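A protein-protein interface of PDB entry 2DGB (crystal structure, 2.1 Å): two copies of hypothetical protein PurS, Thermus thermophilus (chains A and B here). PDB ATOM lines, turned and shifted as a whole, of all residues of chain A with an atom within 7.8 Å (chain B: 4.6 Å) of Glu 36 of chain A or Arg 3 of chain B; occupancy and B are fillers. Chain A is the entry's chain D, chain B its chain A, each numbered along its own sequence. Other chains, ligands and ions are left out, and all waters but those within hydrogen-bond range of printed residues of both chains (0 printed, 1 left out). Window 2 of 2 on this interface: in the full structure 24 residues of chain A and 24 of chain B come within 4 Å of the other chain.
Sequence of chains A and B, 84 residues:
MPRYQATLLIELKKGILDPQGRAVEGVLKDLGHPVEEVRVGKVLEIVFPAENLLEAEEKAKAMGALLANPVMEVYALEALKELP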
ATOM      1  N   ARG A  22       6.621 -28.497 -29.899  1.00  0.00           N
ATOM      2  CA  ARG A  22       6.305 -27.345 -30.734  1.00  0.00           C
ATOM      3  C   ARG A  22       4.801 -27.245 -30.958  1.00  0.00           C
ATOM      4  O   ARG A  22       4.257 -26.145 -31.037  1.00  0.00           O
ATOM      5  CB  ARG A  22       7.037 -27.433 -32.084  1.00  0.00           C
ATOM      6  CG  ARG A  22       8.550 -27.248 -31.983  1.00  0.00           C
ATOM      7  CD  ARG A  22       8.925 -25.829 -31.551  1.00  0.00           C
ATOM      8  NE  ARG A  22       8.589 -24.838 -32.570  1.00  0.00           N
ATOM      9  CZ  ARG A  22       9.321 -24.593 -33.654  1.00  0.00           C
ATOM     10  NH1 ARG A  22      10.447 -25.261 -33.865  1.00  0.00           N
ATOM     11  NH2 ARG A  22       8.922 -23.684 -34.535  1.00  0.00           N
ATOM     12  N   GLU A  25       2.912 -26.005 -27.837  1.00  0.00           N
ATOM     13  CA  GLU A  25       3.085 -24.557 -27.764  1.00  0.00           C
ATOM     14  C   GLU A  25       1.965 -23.899 -28.559  1.00  0.00           C
ATOM     15  O   GLU A  25       1.314 -22.968 -28.081  1.00  0.00           O
ATOM     16  CB  GLU A  25       4.453 -24.142 -28.332  1.00  0.00           C
ATOM     17  CG  GLU A  25       5.605 -24.334 -27.351  1.00  0.00           C
ATOM     18  CD  GLU A  25       6.981 -24.167 -27.987  1.00  0.00           C
ATOM     19  OE1 GLU A  25       7.125 -23.382 -28.950  1.00  0.00           O
ATOM     20  OE2 GLU A  25       7.927 -24.817 -27.509  1.00  0.00           O
ATOM     21  N   LEU A  28      -1.405 -24.175 -26.653  1.00  0.00           N
ATOM     22  CA  LEU A  28      -1.502 -23.253 -25.533  1.00  0.00           C
ATOM     23  C   LEU A  28      -1.625 -21.825 -26.032  1.00  0.00           C
ATOM     24  O   LEU A  28      -2.426 -21.051 -25.510  1.00  0.00           O
ATOM     25  CB  LEU A  28      -0.284 -23.393 -24.616  1.00  0.00           C
ATOM     26  CG  LEU A  28      -0.225 -24.708 -23.837  1.00  0.00           C
ATOM     27  CD1 LEU A  28       1.068 -24.779 -23.031  1.00  0.00           C
ATOM     28  CD2 LEU A  28      -1.438 -24.806 -22.915  1.00  0.00           C
ATOM     29  N   LYS A  29      -0.837 -21.476 -27.048  1.00  0.00           N
ATOM     30  CA  LYS A  29      -0.885 -20.132 -27.608  1.00  0.00           C
ATOM     31  C   LYS A  29      -2.280 -19.832 -28.149  1.00  0.00           C
ATOM     32  O   LYS A  29      -2.767 -18.700 -28.039  1.00  0.00           O
ATOM     33  CB  LYS A  29       0.166 -19.977 -28.709  1.00  0.00           C
ATOM     34  CG  LYS A  29       1.607 -19.920 -28.179  1.00  0.00           C
ATOM     35  CD  LYS A  29       2.622 -20.188 -29.291  1.00  0.00           C
ATOM     36  CE  LYS A  29       4.062 -20.086 -28.797  1.00  0.00           C
ATOM     37  NZ  LYS A  29       4.437 -18.684 -28.437  1.00  0.00           N
ATOM     38  N   HIS A  33      -2.728 -18.738 -23.603  1.00  0.00           N
ATOM     39  CA  HIS A  33      -1.706 -19.022 -22.603  1.00  0.00           C
ATOM     40  C   HIS A  33      -0.307 -18.877 -23.181  1.00  0.00           C
ATOM     41  O   HIS A  33       0.258 -19.827 -23.726  1.00  0.00           O
ATOM     42  CB  HIS A  33      -1.891 -20.427 -22.021  1.00  0.00           C
ATOM     43  CG  HIS A  33      -2.769 -20.462 -20.810  1.00  0.00           C
ATOM     44  ND1 HIS A  33      -4.133 -20.270 -20.872  1.00  0.00           N
ATOM     45  CD2 HIS A  33      -2.469 -20.616 -19.499  1.00  0.00           C
ATOM     46  CE1 HIS A  33      -4.634 -20.302 -19.651  1.00  0.00           C
ATOM     47  NE2 HIS A  33      -3.645 -20.510 -18.799  1.00  0.00           N
ATOM     48  N   PRO A  34       0.266 -17.671 -23.075  1.00  0.00           N
ATOM     49  CA  PRO A  34       1.609 -17.399 -23.590  1.00  0.00           C
ATOM     50  C   PRO A  34       2.636 -18.369 -23.015  1.00  0.00           C
ATOM     51  O   PRO A  34       2.717 -18.548 -21.800  1.00  0.00           O
ATOM     52  CB  PRO A  34       1.866 -15.964 -23.137  1.00  0.00           C
ATOM     53  CG  PRO A  34       0.486 -15.362 -23.139  1.00  0.00           C
ATOM     54  CD  PRO A  34      -0.329 -16.456 -22.492  1.00  0.00           C
ATOM     55  N   VAL A  35       3.405 -19.007 -23.889  1.00  0.00           N
ATOM     56  CA  VAL A  35       4.438 -19.927 -23.445  1.00  0.00           C
ATOM     57  C   VAL A  35       5.710 -19.704 -24.230  1.00  0.00           C
ATOM     58  O   VAL A  35       5.689 -19.498 -25.441  1.00  0.00           O
ATOM     59  CB  VAL A  35       4.033 -21.411 -23.606  1.00  0.00           C
ATOM     60  CG1 VAL A  35       3.042 -21.793 -22.523  1.00  0.00           C
ATOM     61  CG2 VAL A  35       3.445 -21.645 -24.997  1.00  0.00           C
ATOM     62  N   GLU A  36       6.823 -19.743 -23.520  1.00  0.00           N
ATOM     63  CA  GLU A  36       8.112 -19.560 -24.138  1.00  0.00           C
ATOM     64  C   GLU A  36       8.563 -20.878 -24.764  1.00  0.00           C
ATOM     65  O   GLU A  36       9.081 -20.900 -25.879  1.00  0.00           O
ATOM     66  CB  GLU A  36       9.100 -19.082 -23.076  1.00  0.00           C
ATOM     67  CG  GLU A  36      10.547 -19.168 -23.456  1.00  0.00           C
ATOM     68  CD  GLU A  36      11.424 -18.363 -22.514  1.00  0.00           C
ATOM     69  OE1 GLU A  36      12.629 -18.647 -22.461  1.00  0.00           O
ATOM     70  OE2 GLU A  36      10.901 -17.446 -21.840  1.00  0.00           O
ATOM     71  N   GLU A  37       8.335 -21.981 -24.055  1.00  0.00           N
ATOM     72  CA  GLU A  37       8.742 -23.286 -24.555  1.00  0.00           C
ATOM     73  C   GLU A  37       8.015 -24.444 -23.881  1.00  0.00           C
ATOM     74  O   GLU A  37       7.598 -24.344 -22.728  1.00  0.00           O
ATOM     75  CB  GLU A  37      10.249 -23.471 -24.343  1.00  0.00           C
ATOM     76  CG  GLU A  37      10.775 -24.840 -24.758  1.00  0.00           C
ATOM     77  CD  GLU A  37      12.236 -25.052 -24.386  1.00  0.00           C
ATOM     78  OE1 GLU A  37      12.540 -25.175 -23.181  1.00  0.00           O
ATOM     79  OE2 GLU A  37      13.082 -25.093 -25.301  1.00  0.00           O
ATOM     80  N   VAL A  38       7.863 -25.537 -24.623  1.00  0.00           N
ATOM     81  CA  VAL A  38       7.248 -26.750 -24.110  1.00  0.00           C
ATOM     82  C   VAL A  38       8.092 -27.909 -24.625  1.00  0.00           C
ATOM     83  O   VAL A  38       8.206 -28.116 -25.837  1.00  0.00           O
ATOM     84  CB  VAL A  38       5.798 -26.959 -24.617  1.00  0.00           C
ATOM     85  CG1 VAL A  38       5.265 -28.299 -24.098  1.00  0.00           C
ATOM     86  CG2 VAL A  38       4.901 -25.828 -24.141  1.00  0.00           C
ATOM     87  N   PRO B   2       7.711 -12.417 -13.853  1.00  0.00           N
ATOM     88  CA  PRO B   2       8.990 -13.065 -14.227  1.00  0.00           C
ATOM     89  C   PRO B   2       8.745 -14.366 -14.992  1.00  0.00           C
ATOM     90  O   PRO B   2       7.620 -14.645 -15.392  1.00  0.00           O
ATOM     91  CB  PRO B   2       9.752 -13.320 -12.933  1.00  0.00           C
ATOM     92  CG  PRO B   2       8.621 -13.401 -11.929  1.00  0.00           C
ATOM     93  CD  PRO B   2       7.593 -12.354 -12.387  1.00  0.00           C
ATOM     94  N   ARG B   3       9.799 -15.150 -15.200  1.00  0.00           N
ATOM     95  CA  ARG B   3       9.684 -16.411 -15.928  1.00  0.00           C
ATOM     96  C   ARG B   3       9.718 -17.625 -14.999  1.00  0.00           C
ATOM     97  O   ARG B   3      10.407 -17.615 -13.979  1.00  0.00           O
ATOM     98  CB  ARG B   3      10.809 -16.537 -16.959  1.00  0.00           C
ATOM     99  CG  ARG B   3      10.698 -15.616 -18.160  1.00  0.00           C
ATOM    100  CD  ARG B   3      11.637 -16.115 -19.248  1.00  0.00           C
ATOM    101  NE  ARG B   3      12.916 -16.463 -18.656  1.00  0.00           N
ATOM    102  CZ  ARG B   3      13.726 -17.414 -19.096  1.00  0.00           C
ATOM    103  NH1 ARG B   3      13.407 -18.136 -20.160  1.00  0.00           N
ATOM    104  NH2 ARG B   3      14.850 -17.659 -18.441  1.00  0.00           N
ATOM    105  N   TYR B   4       8.989 -18.676 -15.376  1.00  0.00           N
ATOM    106  CA  TYR B   4       8.910 -19.900 -14.577  1.00  0.00           C
ATOM    107  C   TYR B   4       8.948 -21.160 -15.441  1.00  0.00           C
ATOM    108  O   TYR B   4       8.650 -21.124 -16.632  1.00  0.00           O
ATOM    109  CB  TYR B   4       7.600 -19.919 -13.777  1.00  0.00           C
ATOM    110  CG  TYR B   4       7.388 -18.705 -12.900  1.00  0.00           C
ATOM    111  CD1 TYR B   4       7.760 -18.715 -11.559  1.00  0.00           C
ATOM    112  CD2 TYR B   4       6.851 -17.529 -13.427  1.00  0.00           C
ATOM    113  CE1 TYR B   4       7.609 -17.581 -10.759  1.00  0.00           C
ATOM    114  CE2 TYR B   4       6.700 -16.393 -12.642  1.00  0.00           C
ATOM    115  CZ  TYR B   4       7.082 -16.425 -11.311  1.00  0.00           C
ATOM    116  OH  TYR B   4       6.961 -15.289 -10.541  1.00  0.00           O
ATOM    117  N   VAL B  47       8.114 -23.518 -19.955  1.00  0.00           N
ATOM    118  CA  VAL B  47       8.696 -22.239 -19.558  1.00  0.00           C
ATOM    119  C   VAL B  47       7.656 -21.209 -19.989  1.00  0.00           C
ATOM    120  O   VAL B  47       7.264 -21.154 -21.165  1.00  0.00           O
ATOM    121  CB  VAL B  47      10.037 -21.972 -20.285  1.00  0.00           C
ATOM    122  CG1 VAL B  47      10.566 -20.585 -19.928  1.00  0.00           C
ATOM    123  CG2 VAL B  47      11.054 -23.049 -19.896  1.00  0.00           C
ATOM    124  N   PHE B  48       7.199 -20.405 -19.032  1.00  0.00           N
ATOM    125  CA  PHE B  48       6.168 -19.417 -19.301  1.00  0.00           C
ATOM    126  C   PHE B  48       6.250 -18.254 -18.310  1.00  0.00           C
ATOM    127  O   PHE B  48       6.855 -18.383 -17.248  1.00  0.00           O
ATOM    128  CB  PHE B  48       4.804 -20.087 -19.177  1.00  0.00           C
ATOM    129  CG  PHE B  48       4.480 -20.527 -17.776  1.00  0.00           C
ATOM    130  CD1 PHE B  48       3.609 -19.784 -16.985  1.00  0.00           C
ATOM    131  CD2 PHE B  48       5.069 -21.667 -17.236  1.00  0.00           C
ATOM    132  CE1 PHE B  48       3.329 -20.168 -15.672  1.00  0.00           C
ATOM    133  CE2 PHE B  48       4.798 -22.061 -15.920  1.00  0.00           C
ATOM    134  CZ  PHE B  48       3.925 -21.308 -15.139  1.00  0.00           C
ATOM    135  N   PRO B  49       5.606 -17.118 -18.634  1.00  0.00           N
ATOM    136  CA  PRO B  49       5.598 -15.921 -17.784  1.00  0.00           C
ATOM    137  C   PRO B  49       4.428 -15.846 -16.806  1.00  0.00           C
ATOM    138  O   PRO B  49       3.362 -16.424 -17.044  1.00  0.00           O
ATOM    139  CB  PRO B  49       5.528 -14.797 -18.805  1.00  0.00           C
ATOM    140  CG  PRO B  49       4.547 -15.357 -19.781  1.00  0.00           C
ATOM    141  CD  PRO B  49       5.032 -16.804 -19.958  1.00  0.00           C
ATOM    142  N   LYS B  81       9.580 -23.790 -10.726  1.00  0.00           N
ATOM    143  CA  LYS B  81      10.673 -22.937 -10.295  1.00  0.00           C
ATOM    144  C   LYS B  81      10.757 -21.665 -11.107  1.00  0.00           C
ATOM    145  O   LYS B  81      10.400 -21.639 -12.284  1.00  0.00           O
ATOM    146  CB  LYS B  81      12.003 -23.687 -10.393  1.00  0.00           C
ATOM    147  CG  LYS B  81      12.257 -24.316 -11.740  1.00  0.00           C
ATOM    148  CD  LYS B  81      13.618 -25.000 -11.790  1.00  0.00           C
ATOM    149  CE  LYS B  81      14.750 -23.984 -11.699  1.00  0.00           C
ATOM    150  NZ  LYS B  81      16.097 -24.612 -11.851  1.00  0.00           N
ATOM    151  N   GLU B  82      11.226 -20.608 -10.461  1.00  0.00           N
ATOM    152  CA  GLU B  82      11.383 -19.332 -11.123  1.00  0.00           C
ATOM    153  C   GLU B  82      12.704 -19.398 -11.877  1.00  0.00           C
ATOM    154  O   GLU B  82      13.662 -20.017 -11.412  1.00  0.00           O
ATOM    155  CB  GLU B  82      11.430 -18.200 -10.100  1.00  0.00           C
ATOM    156  CG  GLU B  82      11.340 -16.826 -10.730  1.00  0.00           C
ATOM    157  CD  GLU B  82      11.519 -15.717  -9.722  1.00  0.00           C
ATOM    158  OE1 GLU B  82      10.950 -15.822  -8.615  1.00  0.00           O
ATOM    159  OE2 GLU B  82      12.223 -14.740 -10.043  1.00  0.00           O
ATOM    160  N   LEU B  83      12.749 -18.769 -13.043  1.00  0.00           N
ATOM    161  CA  LEU B  83      13.952 -18.771 -13.857  1.00  0.00           C
ATOM    162  C   LEU B  83      14.528 -17.361 -13.903  1.00  0.00           C
ATOM    163  O   LEU B  83      13.844 -16.392 -13.572  1.00  0.00           O
ATOM    164  CB  LEU B  83      13.623 -19.252 -15.271  1.00  0.00           C
ATOM    165  CG  LEU B  83      12.945 -20.623 -15.363  1.00  0.00           C
ATOM    166  CD1 LEU B  83      12.545 -20.909 -16.803  1.00  0.00           C
ATOM    167  CD2 LEU B  83      13.887 -21.696 -14.845  1.00  0.00           C
ATOM    168  N   PRO B  84      15.803 -17.229 -14.296  1.00  0.00           N
ATOM    169  CA  PRO B  84      16.426 -15.905 -14.369  1.00  0.00           C
ATOM    170  C   PRO B  84      15.602 -14.919 -15.204  1.00  0.00           C
ATOM    171  O   PRO B  84      14.750 -15.376 -15.996  1.00  0.00           O
ATOM    172  CB  PRO B  84      17.785 -16.206 -14.996  1.00  0.00           C
ATOM    173  CG  PRO B  84      18.106 -17.548 -14.415  1.00  0.00           C
ATOM    174  CD  PRO B  84      16.791 -18.291 -14.558  1.00  0.00           C
ATOM    175  OXT PRO B  84      15.826 -13.702 -15.066  1.00  0.00           O
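OE1 of Glu 36 of chain A lies within salt-bridge range of NH1 of Arg 3 of chain B (2.5 Å).
The backbone NH of Glu 36 of chain A lies within hydrogen-bond range of the backbone carbonyl oxygen of Val 47 of chain B, at 2.8 Å.
The backbone NH of Val 47 of chain B lies within hydrogen-bond range of the backbone carbonyl oxygen of Glu 37 of chain A, at 2.9 Å.
N of Leu 83 of chain B is in hydrogen-bond range of O of Arg 3 of chain B, 2.8 Å away.
The guanidinium group of Arg 3 of chain B lies within salt-bridge range of the chain-end carboxylate of Pro 84 of chain B, 3.3 Å away.
O of Phe 48 of chain B lies within hydrogen-bond range of N of Tyr 4 of chain B (2.9 Å).
NZ of Lys 29 of chain A is in hydrogen-bond range of O of Val 35 of chain A.
Among the printed residues, merely in contact across the chains: Pro 34 of chain A with Phe 48 of chain B, Pro 34 of chain A with Pro 49 of chain B and Val 35 of chain A with Val 47 of chain B.
Leu 28 of chain A touches none of the printed residues of chain B.
Lys 29 of chain A touches none of the printed residues of chain B.
Of the printed residues of chain B, Pro 34 of chain A touches Phe 48 and Pro 49.
Of the printed residues of chain B, Val 35 of chain A touches Val 47.
Glu 36 of chain A touches just these residues of chain B: Arg 3 and Val 47.
Printed residues of chain B within 4 Å of Glu 37 of chain A: Val 47.
Of chain A, only Glu 36 (2.5 Å) comes within 4 Å of Arg 3 of chain B.
Of the printed residues of chain A, Pro 49 of chain B touches Pro 34.
The nearest residue of chain B that does not touch Glu 36 of chain A is Phe 48 of chain B (4.3 Å).
The nearest residue of chain A that does not touch Arg 3 of chain B is Glu 37 of chain A (7.5 Å).
The nearest printed residue of chain B that does not touch Pro 34 of chain A is Val 47 of chain B (5.3 Å).
Along chain B the printed residues that touch a printed residue of chain A span positions 3 to 49.
Of the 10 printed residues of chain A, 4 touch a printed residue of chain B.
Printed residues of chain A that touch a printed residue of chain B: Pro 34, Val 35, Glu 36 and Glu 37.
Among the printed residues, Asp or Glu carboxylates within 4 Å of a Lys or Arg side-chain nitrogen of the other chain: Glu 36 of chain A with Arg 3 of chain B.
No position is printed for both chains.
Of the 6 pairs that touch across the chains among the printed residues, none has its exchanged pair printed and touching as well.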
